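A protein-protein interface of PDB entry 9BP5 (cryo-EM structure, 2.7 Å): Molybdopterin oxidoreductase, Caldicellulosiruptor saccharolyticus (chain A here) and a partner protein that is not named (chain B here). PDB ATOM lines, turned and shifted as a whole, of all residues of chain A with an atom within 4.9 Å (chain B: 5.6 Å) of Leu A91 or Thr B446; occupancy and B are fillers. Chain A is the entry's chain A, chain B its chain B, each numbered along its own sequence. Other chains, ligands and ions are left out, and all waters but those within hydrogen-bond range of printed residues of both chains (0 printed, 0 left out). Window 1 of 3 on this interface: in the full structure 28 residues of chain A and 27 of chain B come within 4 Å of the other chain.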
ATOM      1  N   ALA A  46      17.168  25.467 -28.984  1.00  0.00           N
ATOM      2  CA  ALA A  46      16.087  25.365 -28.013  1.00  0.00           C
ATOM      3  C   ALA A  46      14.715  25.498 -28.664  1.00  0.00           C
ATOM      4  O   ALA A  46      13.900  24.575 -28.608  1.00  0.00           O
ATOM      5  CB  ALA A  46      16.268  26.430 -26.933  1.00  0.00           C
ATOM      6  N   CYS A  47      14.445  26.644 -29.292  1.00  0.00           N
ATOM      7  CA  CYS A  47      13.081  26.960 -29.706  1.00  0.00           C
ATOM      8  C   CYS A  47      12.553  25.964 -30.732  1.00  0.00           C
ATOM      9  O   CYS A  47      11.386  25.566 -30.675  1.00  0.00           O
ATOM     10  CB  CYS A  47      13.019  28.385 -30.253  1.00  0.00           C
ATOM     11  SG  CYS A  47      13.798  28.623 -31.853  1.00  0.00           S
ATOM     12  N   MET A  87       3.131  23.859 -34.115  1.00  0.00           N
ATOM     13  CA  MET A  87       3.074  23.121 -32.859  1.00  0.00           C
ATOM     14  C   MET A  87       4.047  23.690 -31.837  1.00  0.00           C
ATOM     15  O   MET A  87       3.714  23.798 -30.652  1.00  0.00           O
ATOM     16  CB  MET A  87       3.348  21.641 -33.104  1.00  0.00           C
ATOM     17  CG  MET A  87       3.465  20.822 -31.832  1.00  0.00           C
ATOM     18  SD  MET A  87       1.894  20.511 -31.010  1.00  0.00           S
ATOM     19  CE  MET A  87       0.818  20.264 -32.414  1.00  0.00           C
ATOM     20  N   ALA A  88       5.249  24.075 -32.274  1.00  0.00           N
ATOM     21  CA  ALA A  88       6.197  24.694 -31.353  1.00  0.00           C
ATOM     22  C   ALA A  88       5.654  26.005 -30.801  1.00  0.00           C
ATOM     23  O   ALA A  88       5.798  26.293 -29.607  1.00  0.00           O
ATOM     24  CB  ALA A  88       7.534  24.920 -32.052  1.00  0.00           C
ATOM     25  N   LEU A  89       5.020  26.811 -31.655  1.00  0.00           N
ATOM     26  CA  LEU A  89       4.458  28.078 -31.204  1.00  0.00           C
ATOM     27  C   LEU A  89       3.286  27.869 -30.256  1.00  0.00           C
ATOM     28  O   LEU A  89       3.117  28.627 -29.298  1.00  0.00           O
ATOM     29  CB  LEU A  89       4.031  28.915 -32.406  1.00  0.00           C
ATOM     30  CG  LEU A  89       5.174  29.519 -33.210  1.00  0.00           C
ATOM     31  CD1 LEU A  89       4.650  30.108 -34.497  1.00  0.00           C
ATOM     32  CD2 LEU A  89       5.901  30.562 -32.388  1.00  0.00           C
ATOM     33  N   GLU A  90       2.449  26.865 -30.521  1.00  0.00           N
ATOM     34  CA  GLU A  90       1.351  26.557 -29.610  1.00  0.00           C
ATOM     35  C   GLU A  90       1.876  26.100 -28.257  1.00  0.00           C
ATOM     36  O   GLU A  90       1.330  26.470 -27.211  1.00  0.00           O
ATOM     37  CB  GLU A  90       0.449  25.489 -30.220  1.00  0.00           C
ATOM     38  CG  GLU A  90      -0.486  26.009 -31.284  1.00  0.00           C
ATOM     39  CD  GLU A  90      -1.119  24.896 -32.085  1.00  0.00           C
ATOM     40  OE1 GLU A  90      -1.058  23.734 -31.637  1.00  0.00           O
ATOM     41  OE2 GLU A  90      -1.681  25.182 -33.160  1.00  0.00           O
ATOM     42  N   LEU A  91       2.933  25.290 -28.260  1.00  0.00           N
ATOM     43  CA  LEU A  91       3.555  24.887 -27.006  1.00  0.00           C
ATOM     44  C   LEU A  91       4.111  26.091 -26.258  1.00  0.00           C
ATOM     45  O   LEU A  91       3.972  26.190 -25.036  1.00  0.00           O
ATOM     46  CB  LEU A  91       4.656  23.867 -27.275  1.00  0.00           C
ATOM     47  CG  LEU A  91       4.227  22.459 -27.675  1.00  0.00           C
ATOM     48  CD1 LEU A  91       5.443  21.582 -27.759  1.00  0.00           C
ATOM     49  CD2 LEU A  91       3.227  21.887 -26.695  1.00  0.00           C
ATOM     50  N   LEU A  92       4.742  27.021 -26.974  1.00  0.00           N
ATOM     51  CA  LEU A  92       5.263  28.216 -26.321  1.00  0.00           C
ATOM     52  C   LEU A  92       4.143  29.071 -25.743  1.00  0.00           C
ATOM     53  O   LEU A  92       4.256  29.583 -24.625  1.00  0.00           O
ATOM     54  CB  LEU A  92       6.106  29.021 -27.303  1.00  0.00           C
ATOM     55  CG  LEU A  92       7.524  28.490 -27.461  1.00  0.00           C
ATOM     56  CD1 LEU A  92       8.303  29.334 -28.440  1.00  0.00           C
ATOM     57  CD2 LEU A  92       8.202  28.449 -26.116  1.00  0.00           C
ATOM     58  N   LEU A  93       3.055  29.245 -26.494  1.00  0.00           N
ATOM     59  CA  LEU A  93       1.905  29.992 -26.002  1.00  0.00           C
ATOM     60  C   LEU A  93       1.210  29.286 -24.856  1.00  0.00           C
ATOM     61  O   LEU A  93       0.432  29.915 -24.133  1.00  0.00           O
ATOM     62  CB  LEU A  93       0.897  30.217 -27.119  1.00  0.00           C
ATOM     63  CG  LEU A  93       1.231  31.251 -28.179  1.00  0.00           C
ATOM     64  CD1 LEU A  93       0.187  31.186 -29.268  1.00  0.00           C
ATOM     65  CD2 LEU A  93       1.302  32.630 -27.560  1.00  0.00           C
ATOM     66  N   SER A  94       1.452  27.989 -24.694  1.00  0.00           N
ATOM     67  CA  SER A  94       0.801  27.249 -23.623  1.00  0.00           C
ATOM     68  C   SER A  94       1.210  27.776 -22.251  1.00  0.00           C
ATOM     69  O   SER A  94       0.379  27.857 -21.340  1.00  0.00           O
ATOM     70  CB  SER A  94       1.115  25.763 -23.761  1.00  0.00           C
ATOM     71  OG  SER A  94       0.549  25.254 -24.949  1.00  0.00           O
ATOM     72  N   GLU A  95       2.475  28.149 -22.084  1.00  0.00           N
ATOM     73  CA  GLU A  95       2.994  28.607 -20.802  1.00  0.00           C
ATOM     74  C   GLU A  95       3.138  30.123 -20.740  1.00  0.00           C
ATOM     75  O   GLU A  95       4.007  30.631 -20.027  1.00  0.00           O
ATOM     76  CB  GLU A  95       4.335  27.935 -20.516  1.00  0.00           C
ATOM     77  CG  GLU A  95       5.180  27.715 -21.752  1.00  0.00           C
ATOM     78  CD  GLU A  95       6.659  27.623 -21.441  1.00  0.00           C
ATOM     79  OE1 GLU A  95       7.011  27.058 -20.386  1.00  0.00           O
ATOM     80  OE2 GLU A  95       7.471  28.125 -22.248  1.00  0.00           O
ATOM     81  N   LEU A 590      -3.844  22.661 -26.390  1.00  0.00           N
ATOM     82  CA  LEU A 590      -2.708  22.372 -25.514  1.00  0.00           C
ATOM     83  C   LEU A 590      -2.631  23.363 -24.361  1.00  0.00           C
ATOM     84  O   LEU A 590      -1.599  23.977 -24.111  1.00  0.00           O
ATOM     85  CB  LEU A 590      -1.410  22.376 -26.311  1.00  0.00           C
ATOM     86  CG  LEU A 590      -1.464  21.878 -27.748  1.00  0.00           C
ATOM     87  CD1 LEU A 590      -0.194  22.264 -28.469  1.00  0.00           C
ATOM     88  CD2 LEU A 590      -1.666  20.380 -27.781  1.00  0.00           C
ATOM     89  N   LYS B 444      15.001  22.432 -22.018  1.00  0.00           N
ATOM     90  CA  LYS B 444      15.660  23.384 -22.902  1.00  0.00           C
ATOM     91  C   LYS B 444      14.837  23.684 -24.147  1.00  0.00           C
ATOM     92  O   LYS B 444      14.676  24.852 -24.514  1.00  0.00           O
ATOM     93  CB  LYS B 444      17.045  22.868 -23.307  1.00  0.00           C
ATOM     94  CG  LYS B 444      17.635  23.568 -24.519  1.00  0.00           C
ATOM     95  CD  LYS B 444      18.913  22.895 -24.992  1.00  0.00           C
ATOM     96  CE  LYS B 444      19.999  22.978 -23.938  1.00  0.00           C
ATOM     97  NZ  LYS B 444      21.359  23.066 -24.539  1.00  0.00           N
ATOM     98  N   CYS B 445      14.307  22.656 -24.802  1.00  0.00           N
ATOM     99  CA  CYS B 445      13.519  22.832 -26.013  1.00  0.00           C
ATOM    100  C   CYS B 445      12.037  22.667 -25.706  1.00  0.00           C
ATOM    101  O   CYS B 445      11.645  21.788 -24.935  1.00  0.00           O
ATOM    102  CB  CYS B 445      13.953  21.849 -27.101  1.00  0.00           C
ATOM    103  SG  CYS B 445      13.597  20.133 -26.771  1.00  0.00           S
ATOM    104  N   THR B 446      11.219  23.527 -26.316  1.00  0.00           N
ATOM    105  CA  THR B 446       9.796  23.578 -26.005  1.00  0.00           C
ATOM    106  C   THR B 446       9.066  22.291 -26.354  1.00  0.00           C
ATOM    107  O   THR B 446       8.010  22.017 -25.776  1.00  0.00           O
ATOM    108  CB  THR B 446       9.137  24.742 -26.741  1.00  0.00           C
ATOM    109  OG1 THR B 446       7.714  24.632 -26.631  1.00  0.00           O
ATOM    110  CG2 THR B 446       9.519  24.728 -28.205  1.00  0.00           C
ATOM    111  N   TYR B 447       9.588  21.504 -27.292  1.00  0.00           N
ATOM    112  CA  TYR B 447       8.913  20.273 -27.680  1.00  0.00           C
ATOM    113  C   TYR B 447       8.924  19.257 -26.547  1.00  0.00           C
ATOM    114  O   TYR B 447       7.899  18.641 -26.242  1.00  0.00           O
ATOM    115  CB  TYR B 447       9.569  19.709 -28.933  1.00  0.00           C
ATOM    116  CG  TYR B 447       8.849  20.097 -30.193  1.00  0.00           C
ATOM    117  CD1 TYR B 447       7.467  20.102 -30.244  1.00  0.00           C
ATOM    118  CD2 TYR B 447       9.547  20.496 -31.318  1.00  0.00           C
ATOM    119  CE1 TYR B 447       6.803  20.461 -31.389  1.00  0.00           C
ATOM    120  CE2 TYR B 447       8.888  20.860 -32.473  1.00  0.00           C
ATOM    121  CZ  TYR B 447       7.513  20.842 -32.502  1.00  0.00           C
ATOM    122  OH  TYR B 447       6.845  21.206 -33.645  1.00  0.00           O
ATOM    123  N   CYS B 448      10.079  19.060 -25.916  1.00  0.00           N
ATOM    124  CA  CYS B 448      10.146  18.216 -24.731  1.00  0.00           C
ATOM    125  C   CYS B 448       9.633  18.935 -23.493  1.00  0.00           C
ATOM    126  O   CYS B 448       9.039  18.302 -22.616  1.00  0.00           O
ATOM    127  CB  CYS B 448      11.582  17.746 -24.499  1.00  0.00           C
ATOM    128  SG  CYS B 448      11.805  16.637 -23.093  1.00  0.00           S
ATOM    129  N   ARG B 449       9.848  20.247 -23.404  1.00  0.00           N
ATOM    130  CA  ARG B 449       9.505  20.969 -22.185  1.00  0.00           C
ATOM    131  C   ARG B 449       7.999  21.126 -22.030  1.00  0.00           C
ATOM    132  O   ARG B 449       7.468  20.985 -20.922  1.00  0.00           O
ATOM    133  CB  ARG B 449      10.185  22.335 -22.182  1.00  0.00           C
ATOM    134  CG  ARG B 449      10.293  22.974 -20.818  1.00  0.00           C
ATOM    135  CD  ARG B 449      11.116  24.247 -20.883  1.00  0.00           C
ATOM    136  NE  ARG B 449      10.399  25.321 -21.559  1.00  0.00           N
ATOM    137  CZ  ARG B 449      10.669  25.746 -22.785  1.00  0.00           C
ATOM    138  NH1 ARG B 449      11.640  25.210 -23.505  1.00  0.00           N
ATOM    139  NH2 ARG B 449       9.945  26.735 -23.303  1.00  0.00           N
ATOM    140  N   VAL B 450       7.296  21.424 -23.118  1.00  0.00           N
ATOM    141  CA  VAL B 450       5.865  21.679 -23.076  1.00  0.00           C
ATOM    142  C   VAL B 450       5.067  20.529 -23.676  1.00  0.00           C
ATOM    143  O   VAL B 450       3.996  20.187 -23.169  1.00  0.00           O
ATOM    144  CB  VAL B 450       5.521  23.008 -23.780  1.00  0.00           C
ATOM    145  CG1 VAL B 450       4.134  23.470 -23.370  1.00  0.00           C
ATOM    146  CG2 VAL B 450       6.560  24.066 -23.453  1.00  0.00           C
ATOM    147  N   GLY B 451       5.564  19.927 -24.756  1.00  0.00           N
ATOM    148  CA  GLY B 451       4.829  18.844 -25.386  1.00  0.00           C
ATOM    149  C   GLY B 451       4.626  17.662 -24.460  1.00  0.00           C
ATOM    150  O   GLY B 451       3.531  17.100 -24.388  1.00  0.00           O
ATOM    151  N   ARG B 454       2.071  18.631 -21.787  1.00  0.00           N
ATOM    152  CA  ARG B 454       0.712  18.659 -22.322  1.00  0.00           C
ATOM    153  C   ARG B 454       0.185  17.252 -22.577  1.00  0.00           C
ATOM    154  O   ARG B 454      -0.990  16.965 -22.314  1.00  0.00           O
ATOM    155  CB  ARG B 454       0.669  19.495 -23.598  1.00  0.00           C
ATOM    156  CG  ARG B 454       0.807  20.992 -23.359  1.00  0.00           C
ATOM    157  CD  ARG B 454       0.063  21.422 -22.104  1.00  0.00           C
ATOM    158  NE  ARG B 454       0.013  22.872 -21.962  1.00  0.00           N
ATOM    159  CZ  ARG B 454      -0.033  23.510 -20.801  1.00  0.00           C
ATOM    160  NH1 ARG B 454      -0.042  22.854 -19.652  1.00  0.00           N
ATOM    161  NH2 ARG B 454      -0.074  24.839 -20.792  1.00  0.00           N
ATOM    162  N   LEU B 478       0.286  15.218 -30.970  1.00  0.00           N
ATOM    163  CA  LEU B 478       1.313  15.688 -30.044  1.00  0.00           C
ATOM    164  C   LEU B 478       2.495  14.735 -30.003  1.00  0.00           C
ATOM    165  O   LEU B 478       3.649  15.172 -29.986  1.00  0.00           O
ATOM    166  CB  LEU B 478       0.740  15.857 -28.640  1.00  0.00           C
ATOM    167  CG  LEU B 478       0.437  17.280 -28.185  1.00  0.00           C
ATOM    168  CD1 LEU B 478      -0.043  17.279 -26.750  1.00  0.00           C
ATOM    169  CD2 LEU B 478       1.677  18.134 -28.326  1.00  0.00           C
ATOM    170  N   VAL B 482       6.225  15.850 -31.072  1.00  0.00           N
ATOM    171  CA  VAL B 482       7.290  15.813 -30.077  1.00  0.00           C
ATOM    172  C   VAL B 482       8.403  14.877 -30.523  1.00  0.00           C
ATOM    173  O   VAL B 482       9.588  15.150 -30.303  1.00  0.00           O
ATOM    174  CB  VAL B 482       6.713  15.405 -28.710  1.00  0.00           C
ATOM    175  CG1 VAL B 482       7.814  14.982 -27.765  1.00  0.00           C
ATOM    176  CG2 VAL B 482       5.913  16.546 -28.117  1.00  0.00           C
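O of Lys B444 is in hydrogen-bond range of NH1 of Arg B449 (3.2 Å).
O of Glu A90 is in hydrogen-bond range of OG of Ser A94 (2.7 Å).
The side-chain hydroxyl (OG) of Ser A94 is in hydrogen-bond range of the backbone carbonyl oxygen (O) of Leu A590, 2.6 Å away.
The backbone carbonyl oxygen (O) of Thr B446 lies within hydrogen-bond range of the backbone NH (N) of Gly B451 (3.4 Å).
SG of Cys B445 sits close to N of Cys B448, 3.8 Å away.
Of the 11 printed residues of chain B, 9 touch a printed residue of chain A.
Printed residues of chain B that touch a printed residue of chain A: Lys B444, Cys B445, Thr B446, Tyr B447, Arg B449, Val B450, Gly B451, Arg B454 and Leu B478.
Hydrophobic or aromatic side chains of chain B within 4 Å of the printed part of chain A: Tyr B447, Val B450 and Leu B478.
Of the 12 printed residues of chain A, 9 touch a printed residue of chain B.
Hydrophobic or aromatic side chains of chain A within 4 Å of the printed part of chain B: Ala A46, Met A87, Leu A91, Leu A92 and Leu A590.
Among the printed residues, 19 pairs touch across the chains.
Leu A89 touches none of the printed residues of chain B.
Of chain B, only Thr B446, Tyr B447, Val B450 and Gly B451 come within 4 Å of Leu A91.
Printed residues of chain B within 4 Å of Leu A92: Thr B446 and Arg B449.
Leu A93 touches none of the printed residues of chain B.
Printed residues of chain B within 4 Å of Ser A94: Val B450 (3.8 Å) and Arg B454 (3.1 Å).
Thr B446 touches just these residues of chain A: Ala A46 (3.7 Å), Cys A47 (3.2 Å), Ala A88 (3.9 Å), Leu A91 (3.2 Å) and Leu A92 (3.8 Å).
Of the printed residues of chain A, Tyr B447 touches Met A87 (3.4 Å), Ala A88 (3.6 Å) and Leu A91 (3.5 Å).
Printed residues of chain A within 4 Å of Arg B449: Leu A92 and Glu A95.
The nearest residue of chain B that does not touch Leu A91 is Arg B454 (4.2 Å).
The nearest printed residue of chain A that does not touch Thr B446 is Glu A95 (5.6 Å).
OE2 of Glu A95 lies within salt-bridge range of NH2 of Arg B449 (3.0 Å).
O of Leu A590 is in hydrogen-bond range of NE of Arg B454 (2.9 Å).
The backbone carbonyl oxygen (O) of Ser A94 sits at hydrogen-bond distance from the guanidinium group (NH2) of Arg B454.
Among the printed residues, pairs that only touch across the chains: Ala A46 with Lys B444, Ala A46 with Cys B445, Ala A46 with Thr B446, Cys A47 with Thr B446, Met A87 with Tyr B447, Met A87 with Leu B478, Ala A88 with Thr B446, Ala A88 with Tyr B447, Leu A91 with Thr B446, Leu A91 with Tyr B447, Leu A91 with Val B450, Leu A91 with Gly B451, Leu A92 with Thr B446, Leu A92 with Arg B449, Ser A94 with Val B450 and Leu A590 with Leu B478.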
